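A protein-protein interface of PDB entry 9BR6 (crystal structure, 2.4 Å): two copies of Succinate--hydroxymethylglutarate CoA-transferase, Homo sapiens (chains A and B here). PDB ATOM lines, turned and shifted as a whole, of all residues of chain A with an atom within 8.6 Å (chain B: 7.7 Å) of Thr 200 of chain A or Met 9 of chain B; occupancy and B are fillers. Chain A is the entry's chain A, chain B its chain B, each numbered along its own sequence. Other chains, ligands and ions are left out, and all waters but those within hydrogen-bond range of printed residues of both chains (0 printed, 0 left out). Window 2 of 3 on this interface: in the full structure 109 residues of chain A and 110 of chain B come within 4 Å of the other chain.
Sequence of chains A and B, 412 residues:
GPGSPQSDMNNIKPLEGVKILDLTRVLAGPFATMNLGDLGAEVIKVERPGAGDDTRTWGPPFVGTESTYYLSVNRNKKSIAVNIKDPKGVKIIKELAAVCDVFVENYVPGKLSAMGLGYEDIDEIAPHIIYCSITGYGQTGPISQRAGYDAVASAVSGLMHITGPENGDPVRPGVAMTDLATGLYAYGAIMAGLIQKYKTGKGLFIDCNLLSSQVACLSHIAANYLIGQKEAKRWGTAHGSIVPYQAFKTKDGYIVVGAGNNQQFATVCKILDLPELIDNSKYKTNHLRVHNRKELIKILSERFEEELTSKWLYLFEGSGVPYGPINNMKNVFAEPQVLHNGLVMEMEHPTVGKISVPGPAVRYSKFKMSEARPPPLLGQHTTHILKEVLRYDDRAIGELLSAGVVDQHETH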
ATOM      1  N   PRO A 127      -8.311  -8.437  23.892  1.00  0.00           N
ATOM      2  CA  PRO A 127      -8.408  -9.806  23.357  1.00  0.00           C
ATOM      3  C   PRO A 127      -8.766  -9.848  21.885  1.00  0.00           C
ATOM      4  O   PRO A 127      -8.448 -10.828  21.202  1.00  0.00           O
ATOM      5  CB  PRO A 127      -9.497 -10.447  24.227  1.00  0.00           C
ATOM      6  CG  PRO A 127     -10.307  -9.302  24.721  1.00  0.00           C
ATOM      7  CD  PRO A 127      -9.342  -8.168  24.911  1.00  0.00           C
ATOM      8  N   HIS A 128      -9.469  -8.828  21.396  1.00  0.00           N
ATOM      9  CA  HIS A 128      -9.814  -8.728  19.985  1.00  0.00           C
ATOM     10  C   HIS A 128      -8.606  -8.461  19.096  1.00  0.00           C
ATOM     11  O   HIS A 128      -8.653  -8.776  17.902  1.00  0.00           O
ATOM     12  CB  HIS A 128     -10.825  -7.602  19.796  1.00  0.00           C
ATOM     13  CG  HIS A 128     -10.332  -6.279  20.297  1.00  0.00           C
ATOM     14  ND1 HIS A 128     -10.362  -5.938  21.633  1.00  0.00           N
ATOM     15  CD2 HIS A 128      -9.741  -5.240  19.658  1.00  0.00           C
ATOM     16  CE1 HIS A 128      -9.843  -4.732  21.790  1.00  0.00           C
ATOM     17  NE2 HIS A 128      -9.458  -4.288  20.608  1.00  0.00           N
ATOM     18  N   ILE A 130      -5.372  -8.017  16.795  1.00  0.00           N
ATOM     19  CA  ILE A 130      -4.561  -8.866  15.932  1.00  0.00           C
ATOM     20  C   ILE A 130      -3.115  -8.413  16.078  1.00  0.00           C
ATOM     21  O   ILE A 130      -2.755  -7.307  15.660  1.00  0.00           O
ATOM     22  CB  ILE A 130      -5.019  -8.803  14.470  1.00  0.00           C
ATOM     23  CG1 ILE A 130      -6.505  -9.139  14.362  1.00  0.00           C
ATOM     24  CG2 ILE A 130      -4.193  -9.754  13.616  1.00  0.00           C
ATOM     25  CD1 ILE A 130      -6.830 -10.582  14.643  1.00  0.00           C
ATOM     26  N   GLY A 193      -6.090 -12.414   9.593  1.00  0.00           N
ATOM     27  CA  GLY A 193      -6.490 -12.329  10.989  1.00  0.00           C
ATOM     28  C   GLY A 193      -7.789 -11.572  11.193  1.00  0.00           C
ATOM     29  O   GLY A 193      -8.609 -11.945  12.035  1.00  0.00           O
ATOM     30  N   LEU A 194      -7.988 -10.491  10.434  1.00  0.00           N
ATOM     31  CA  LEU A 194      -9.229  -9.727  10.548  1.00  0.00           C
ATOM     32  C   LEU A 194     -10.433 -10.559  10.122  1.00  0.00           C
ATOM     33  O   LEU A 194     -11.495 -10.496  10.754  1.00  0.00           O
ATOM     34  CB  LEU A 194      -9.136  -8.443   9.722  1.00  0.00           C
ATOM     35  CG  LEU A 194      -8.171  -7.359  10.214  1.00  0.00           C
ATOM     36  CD1 LEU A 194      -8.163  -6.198   9.242  1.00  0.00           C
ATOM     37  CD2 LEU A 194      -8.539  -6.880  11.615  1.00  0.00           C
ATOM     38  N   ILE A 195     -10.291 -11.343   9.050  1.00  0.00           N
ATOM     39  CA  ILE A 195     -11.382 -12.206   8.604  1.00  0.00           C
ATOM     40  C   ILE A 195     -11.696 -13.266   9.654  1.00  0.00           C
ATOM     41  O   ILE A 195     -12.865 -13.557   9.935  1.00  0.00           O
ATOM     42  CB  ILE A 195     -11.035 -12.841   7.245  1.00  0.00           C
ATOM     43  CG1 ILE A 195     -10.881 -11.753   6.181  1.00  0.00           C
ATOM     44  CG2 ILE A 195     -12.091 -13.863   6.840  1.00  0.00           C
ATOM     45  CD1 ILE A 195     -10.632 -12.285   4.791  1.00  0.00           C
ATOM     46  N   GLN A 196     -10.657 -13.863  10.244  1.00  0.00           N
ATOM     47  CA  GLN A 196     -10.867 -14.831  11.316  1.00  0.00           C
ATOM     48  C   GLN A 196     -11.491 -14.174  12.541  1.00  0.00           C
ATOM     49  O   GLN A 196     -12.343 -14.772  13.210  1.00  0.00           O
ATOM     50  CB  GLN A 196      -9.542 -15.506  11.673  1.00  0.00           C
ATOM     51  CG  GLN A 196      -9.561 -16.320  12.955  1.00  0.00           C
ATOM     52  CD  GLN A 196     -10.083 -17.728  12.740  1.00  0.00           C
ATOM     53  OE1 GLN A 196     -10.475 -18.095  11.631  1.00  0.00           O
ATOM     54  NE2 GLN A 196     -10.072 -18.533  13.798  1.00  0.00           N
ATOM     55  N   LYS A 197     -11.073 -12.945  12.857  1.00  0.00           N
ATOM     56  CA  LYS A 197     -11.623 -12.244  14.013  1.00  0.00           C
ATOM     57  C   LYS A 197     -13.115 -11.981  13.840  1.00  0.00           C
ATOM     58  O   LYS A 197     -13.875 -12.027  14.812  1.00  0.00           O
ATOM     59  CB  LYS A 197     -10.867 -10.937  14.249  1.00  0.00           C
ATOM     60  CG  LYS A 197     -11.499 -10.017  15.284  1.00  0.00           C
ATOM     61  CD  LYS A 197     -10.750  -8.700  15.340  1.00  0.00           C
ATOM     62  CE  LYS A 197     -11.467  -7.664  16.187  1.00  0.00           C
ATOM     63  NZ  LYS A 197     -10.713  -6.378  16.176  1.00  0.00           N
ATOM     64  N   TYR A 198     -13.548 -11.680  12.612  1.00  0.00           N
ATOM     65  CA  TYR A 198     -14.969 -11.451  12.365  1.00  0.00           C
ATOM     66  C   TYR A 198     -15.787 -12.692  12.710  1.00  0.00           C
ATOM     67  O   TYR A 198     -16.882 -12.587  13.274  1.00  0.00           O
ATOM     68  CB  TYR A 198     -15.195 -11.046  10.909  1.00  0.00           C
ATOM     69  CG  TYR A 198     -14.495  -9.762  10.510  1.00  0.00           C
ATOM     70  CD1 TYR A 198     -14.259  -8.752  11.437  1.00  0.00           C
ATOM     71  CD2 TYR A 198     -14.057  -9.566   9.204  1.00  0.00           C
ATOM     72  CE1 TYR A 198     -13.611  -7.584  11.075  1.00  0.00           C
ATOM     73  CE2 TYR A 198     -13.410  -8.400   8.832  1.00  0.00           C
ATOM     74  CZ  TYR A 198     -13.188  -7.415   9.771  1.00  0.00           C
ATOM     75  OH  TYR A 198     -12.546  -6.254   9.403  1.00  0.00           O
ATOM     76  N   LYS A 199     -15.277 -13.876  12.361  1.00  0.00           N
ATOM     77  CA  LYS A 199     -15.991 -15.113  12.657  1.00  0.00           C
ATOM     78  C   LYS A 199     -15.962 -15.428  14.149  1.00  0.00           C
ATOM     79  O   LYS A 199     -17.007 -15.676  14.763  1.00  0.00           O
ATOM     80  CB  LYS A 199     -15.382 -16.271  11.866  1.00  0.00           C
ATOM     81  CG  LYS A 199     -15.307 -16.062  10.365  1.00  0.00           C
ATOM     82  CD  LYS A 199     -14.645 -17.262   9.711  1.00  0.00           C
ATOM     83  CE  LYS A 199     -14.631 -17.157   8.199  1.00  0.00           C
ATOM     84  NZ  LYS A 199     -14.007 -18.373   7.599  1.00  0.00           N
ATOM     85  N   THR A 200     -14.769 -15.425  14.749  1.00  0.00           N
ATOM     86  CA  THR A 200     -14.589 -15.868  16.127  1.00  0.00           C
ATOM     87  C   THR A 200     -14.852 -14.783  17.163  1.00  0.00           C
ATOM     88  O   THR A 200     -15.345 -15.090  18.255  1.00  0.00           O
ATOM     89  CB  THR A 200     -13.168 -16.411  16.325  1.00  0.00           C
ATOM     90  OG1 THR A 200     -12.233 -15.325  16.309  1.00  0.00           O
ATOM     91  CG2 THR A 200     -12.817 -17.410  15.231  1.00  0.00           C
ATOM     92  N   GLY A 201     -14.537 -13.530  16.860  1.00  0.00           N
ATOM     93  CA  GLY A 201     -14.655 -12.468  17.837  1.00  0.00           C
ATOM     94  C   GLY A 201     -13.460 -12.291  18.743  1.00  0.00           C
ATOM     95  O   GLY A 201     -13.535 -11.501  19.693  1.00  0.00           O
ATOM     96  N   LYS A 202     -12.366 -13.004  18.492  1.00  0.00           N
ATOM     97  CA  LYS A 202     -11.150 -12.877  19.279  1.00  0.00           C
ATOM     98  C   LYS A 202      -9.955 -12.739  18.346  1.00  0.00           C
ATOM     99  O   LYS A 202      -9.987 -13.187  17.197  1.00  0.00           O
ATOM    100  CB  LYS A 202     -10.951 -14.069  20.239  1.00  0.00           C
ATOM    101  CG  LYS A 202     -11.964 -14.121  21.380  1.00  0.00           C
ATOM    102  CD  LYS A 202     -11.666 -15.251  22.356  1.00  0.00           C
ATOM    103  CE  LYS A 202     -12.773 -15.394  23.394  1.00  0.00           C
ATOM    104  NZ  LYS A 202     -12.536 -16.535  24.328  1.00  0.00           N
ATOM    105  N   GLY A 203      -8.912 -12.079  18.845  1.00  0.00           N
ATOM    106  CA  GLY A 203      -7.705 -11.881  18.075  1.00  0.00           C
ATOM    107  C   GLY A 203      -6.756 -13.061  18.131  1.00  0.00           C
ATOM    108  O   GLY A 203      -6.955 -14.034  18.857  1.00  0.00           O
ATOM    109  N   LEU A 204      -5.704 -12.970  17.323  1.00  0.00           N
ATOM    110  CA  LEU A 204      -4.683 -14.004  17.250  1.00  0.00           C
ATOM    111  C   LEU A 204      -3.316 -13.356  17.080  1.00  0.00           C
ATOM    112  O   LEU A 204      -3.196 -12.149  16.850  1.00  0.00           O
ATOM    113  CB  LEU A 204      -4.987 -14.999  16.122  1.00  0.00           C
ATOM    114  CG  LEU A 204      -5.192 -14.509  14.687  1.00  0.00           C
ATOM    115  CD1 LEU A 204      -3.884 -14.266  13.971  1.00  0.00           C
ATOM    116  CD2 LEU A 204      -6.032 -15.521  13.929  1.00  0.00           C
ATOM    117  N   ASP B   8     -16.337 -24.694  18.999  1.00  0.00           N
ATOM    118  CA  ASP B   8     -16.100 -25.330  17.710  1.00  0.00           C
ATOM    119  C   ASP B   8     -15.307 -24.392  16.802  1.00  0.00           C
ATOM    120  O   ASP B   8     -14.715 -24.822  15.811  1.00  0.00           O
ATOM    121  CB  ASP B   8     -17.426 -25.726  17.054  1.00  0.00           C
ATOM    122  CG  ASP B   8     -17.274 -26.856  16.051  1.00  0.00           C
ATOM    123  OD1 ASP B   8     -16.127 -27.258  15.763  1.00  0.00           O
ATOM    124  OD2 ASP B   8     -18.307 -27.352  15.555  1.00  0.00           O
ATOM    125  N   MET B   9     -15.297 -23.107  17.154  1.00  0.00           N
ATOM    126  CA  MET B   9     -14.559 -22.092  16.416  1.00  0.00           C
ATOM    127  C   MET B   9     -13.172 -21.835  16.996  1.00  0.00           C
ATOM    128  O   MET B   9     -12.509 -20.879  16.581  1.00  0.00           O
ATOM    129  CB  MET B   9     -15.349 -20.780  16.384  1.00  0.00           C
ATOM    130  CG  MET B   9     -16.862 -20.954  16.399  1.00  0.00           C
ATOM    131  SD  MET B   9     -17.515 -21.858  14.980  1.00  0.00           S
ATOM    132  CE  MET B   9     -17.148 -20.722  13.646  1.00  0.00           C
ATOM    133  N   ASN B  10     -12.729 -22.663  17.946  1.00  0.00           N
ATOM    134  CA  ASN B  10     -11.435 -22.443  18.586  1.00  0.00           C
ATOM    135  C   ASN B  10     -10.298 -22.558  17.580  1.00  0.00           C
ATOM    136  O   ASN B  10      -9.380 -21.728  17.560  1.00  0.00           O
ATOM    137  CB  ASN B  10     -11.232 -23.448  19.723  1.00  0.00           C
ATOM    138  CG  ASN B  10     -12.468 -23.621  20.581  1.00  0.00           C
ATOM    139  OD1 ASN B  10     -13.594 -23.473  20.107  1.00  0.00           O
ATOM    140  ND2 ASN B  10     -12.263 -23.943  21.853  1.00  0.00           N
ATOM    141  N   ASN B  11     -10.347 -23.581  16.731  1.00  0.00           N
ATOM    142  CA  ASN B  11      -9.231 -23.958  15.872  1.00  0.00           C
ATOM    143  C   ASN B  11      -9.741 -24.100  14.432  1.00  0.00           C
ATOM    144  O   ASN B  11      -9.873 -25.208  13.910  1.00  0.00           O
ATOM    145  CB  ASN B  11      -8.585 -25.251  16.374  1.00  0.00           C
ATOM    146  CG  ASN B  11      -7.982 -25.111  17.761  1.00  0.00           C
ATOM    147  OD1 ASN B  11      -8.481 -25.685  18.730  1.00  0.00           O
ATOM    148  ND2 ASN B  11      -6.892 -24.357  17.860  1.00  0.00           N
ATOM    149  N   ILE B  12     -10.021 -22.968  13.788  1.00  0.00           N
ATOM    150  CA  ILE B  12     -10.570 -22.946  12.437  1.00  0.00           C
ATOM    151  C   ILE B  12      -9.773 -21.962  11.589  1.00  0.00           C
ATOM    152  O   ILE B  12      -9.333 -20.917  12.081  1.00  0.00           O
ATOM    153  CB  ILE B  12     -12.073 -22.582  12.444  1.00  0.00           C
ATOM    154  CG1 ILE B  12     -12.642 -22.607  11.024  1.00  0.00           C
ATOM    155  CG2 ILE B  12     -12.299 -21.229  13.115  1.00  0.00           C
ATOM    156  CD1 ILE B  12     -14.143 -22.435  10.955  1.00  0.00           C
ATOM    157  N   LYS B  13      -9.581 -22.305  10.306  1.00  0.00           N
ATOM    158  CA  LYS B  13      -8.789 -21.489   9.400  1.00  0.00           C
ATOM    159  C   LYS B  13      -9.618 -20.329   8.840  1.00  0.00           C
ATOM    160  O   LYS B  13     -10.832 -20.454   8.658  1.00  0.00           O
ATOM    161  CB  LYS B  13      -8.240 -22.346   8.261  1.00  0.00           C
ATOM    162  CG  LYS B  13      -7.164 -23.341   8.694  1.00  0.00           C
ATOM    163  CD  LYS B  13      -6.480 -23.983   7.493  1.00  0.00           C
ATOM    164  CE  LYS B  13      -5.318 -24.879   7.910  1.00  0.00           C
ATOM    165  NZ  LYS B  13      -4.637 -25.484   6.725  1.00  0.00           N
ATOM    166  N   LYS B 366      -3.673 -19.315  16.383  1.00  0.00           N
ATOM    167  CA  LYS B 366      -4.956 -20.004  16.543  1.00  0.00           C
ATOM    168  C   LYS B 366      -5.012 -21.313  15.762  1.00  0.00           C
ATOM    169  O   LYS B 366      -5.688 -22.258  16.183  1.00  0.00           O
ATOM    170  CB  LYS B 366      -6.109 -19.100  16.108  1.00  0.00           C
ATOM    171  CG  LYS B 366      -6.409 -17.940  17.033  1.00  0.00           C
ATOM    172  CD  LYS B 366      -6.840 -18.391  18.409  1.00  0.00           C
ATOM    173  CE  LYS B 366      -7.207 -17.192  19.268  1.00  0.00           C
ATOM    174  NZ  LYS B 366      -7.776 -17.594  20.585  1.00  0.00           N
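The side-chain amide nitrogen (NE2) of Gln 196 of chain A sits at hydrogen-bond distance from the backbone carbonyl oxygen (O) of Ile 12 of chain B (3.0 Å).
Hydrophobic or aromatic side chains of chain B within 4 Å of the printed part of chain A: Ile 12.
Printed residues of chain A that touch a printed residue of chain B: Gln 196, Lys 199, Thr 200, Gly 203 and Leu 204.
Among the printed residues, no Asp or Glu carboxylate lies within 4 Å of a Lys or Arg side-chain nitrogen of the other chain.
Among the printed residues, merely in contact across the chains: Gly 203 of chain A with Lys 366 of chain B, Leu 204 of chain A with Lys 366 of chain B, Gln 196 of chain A with Lys 13 of chain B, Thr 200 of chain A with Met 9 of chain B and Lys 199 of chain A with Lys 13 of chain B.
The backbone carbonyl oxygen (O) of Pro 127 of chain A sits at hydrogen-bond distance from the backbone NH (N) of Gly 203 of chain A (2.7 Å).
O of His 128 of chain A sits close to N of Gly 203 of chain A.
OG1 of Thr 200 of chain A sits at hydrogen-bond distance from O of Gln 196 of chain A.
N of Lys 202 of chain A lies within hydrogen-bond range of OG1 of Thr 200 of chain A.
ND2 of Asn 11 of chain B lies within hydrogen-bond range of O of Lys 366 of chain B (2.9 Å).
Thr 200 of chain A touches one residue of chain B.
Of chain A, only Thr 200 (3.7 Å) comes within 4 Å of Met 9 of chain B.
Printed residues of chain B within 4 Å of Gly 203 of chain A: Lys 366.
Of the printed residues of chain A, Ile 12 of chain B touches Gln 196 (3.0 Å).
Printed residues of chain B within 4 Å of Gln 196 of chain A: Ile 12 and Lys 13.
Of the printed residues of chain B, Leu 204 of chain A touches Lys 366 (3.4 Å).
The nearest residue of chain A that does not touch Met 9 of chain B is Gln 196 of chain A (4.4 Å).
No position is printed for both chains.
Of the 6 pairs that touch across the chains among the printed residues, none has its exchanged pair printed and touching as well.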
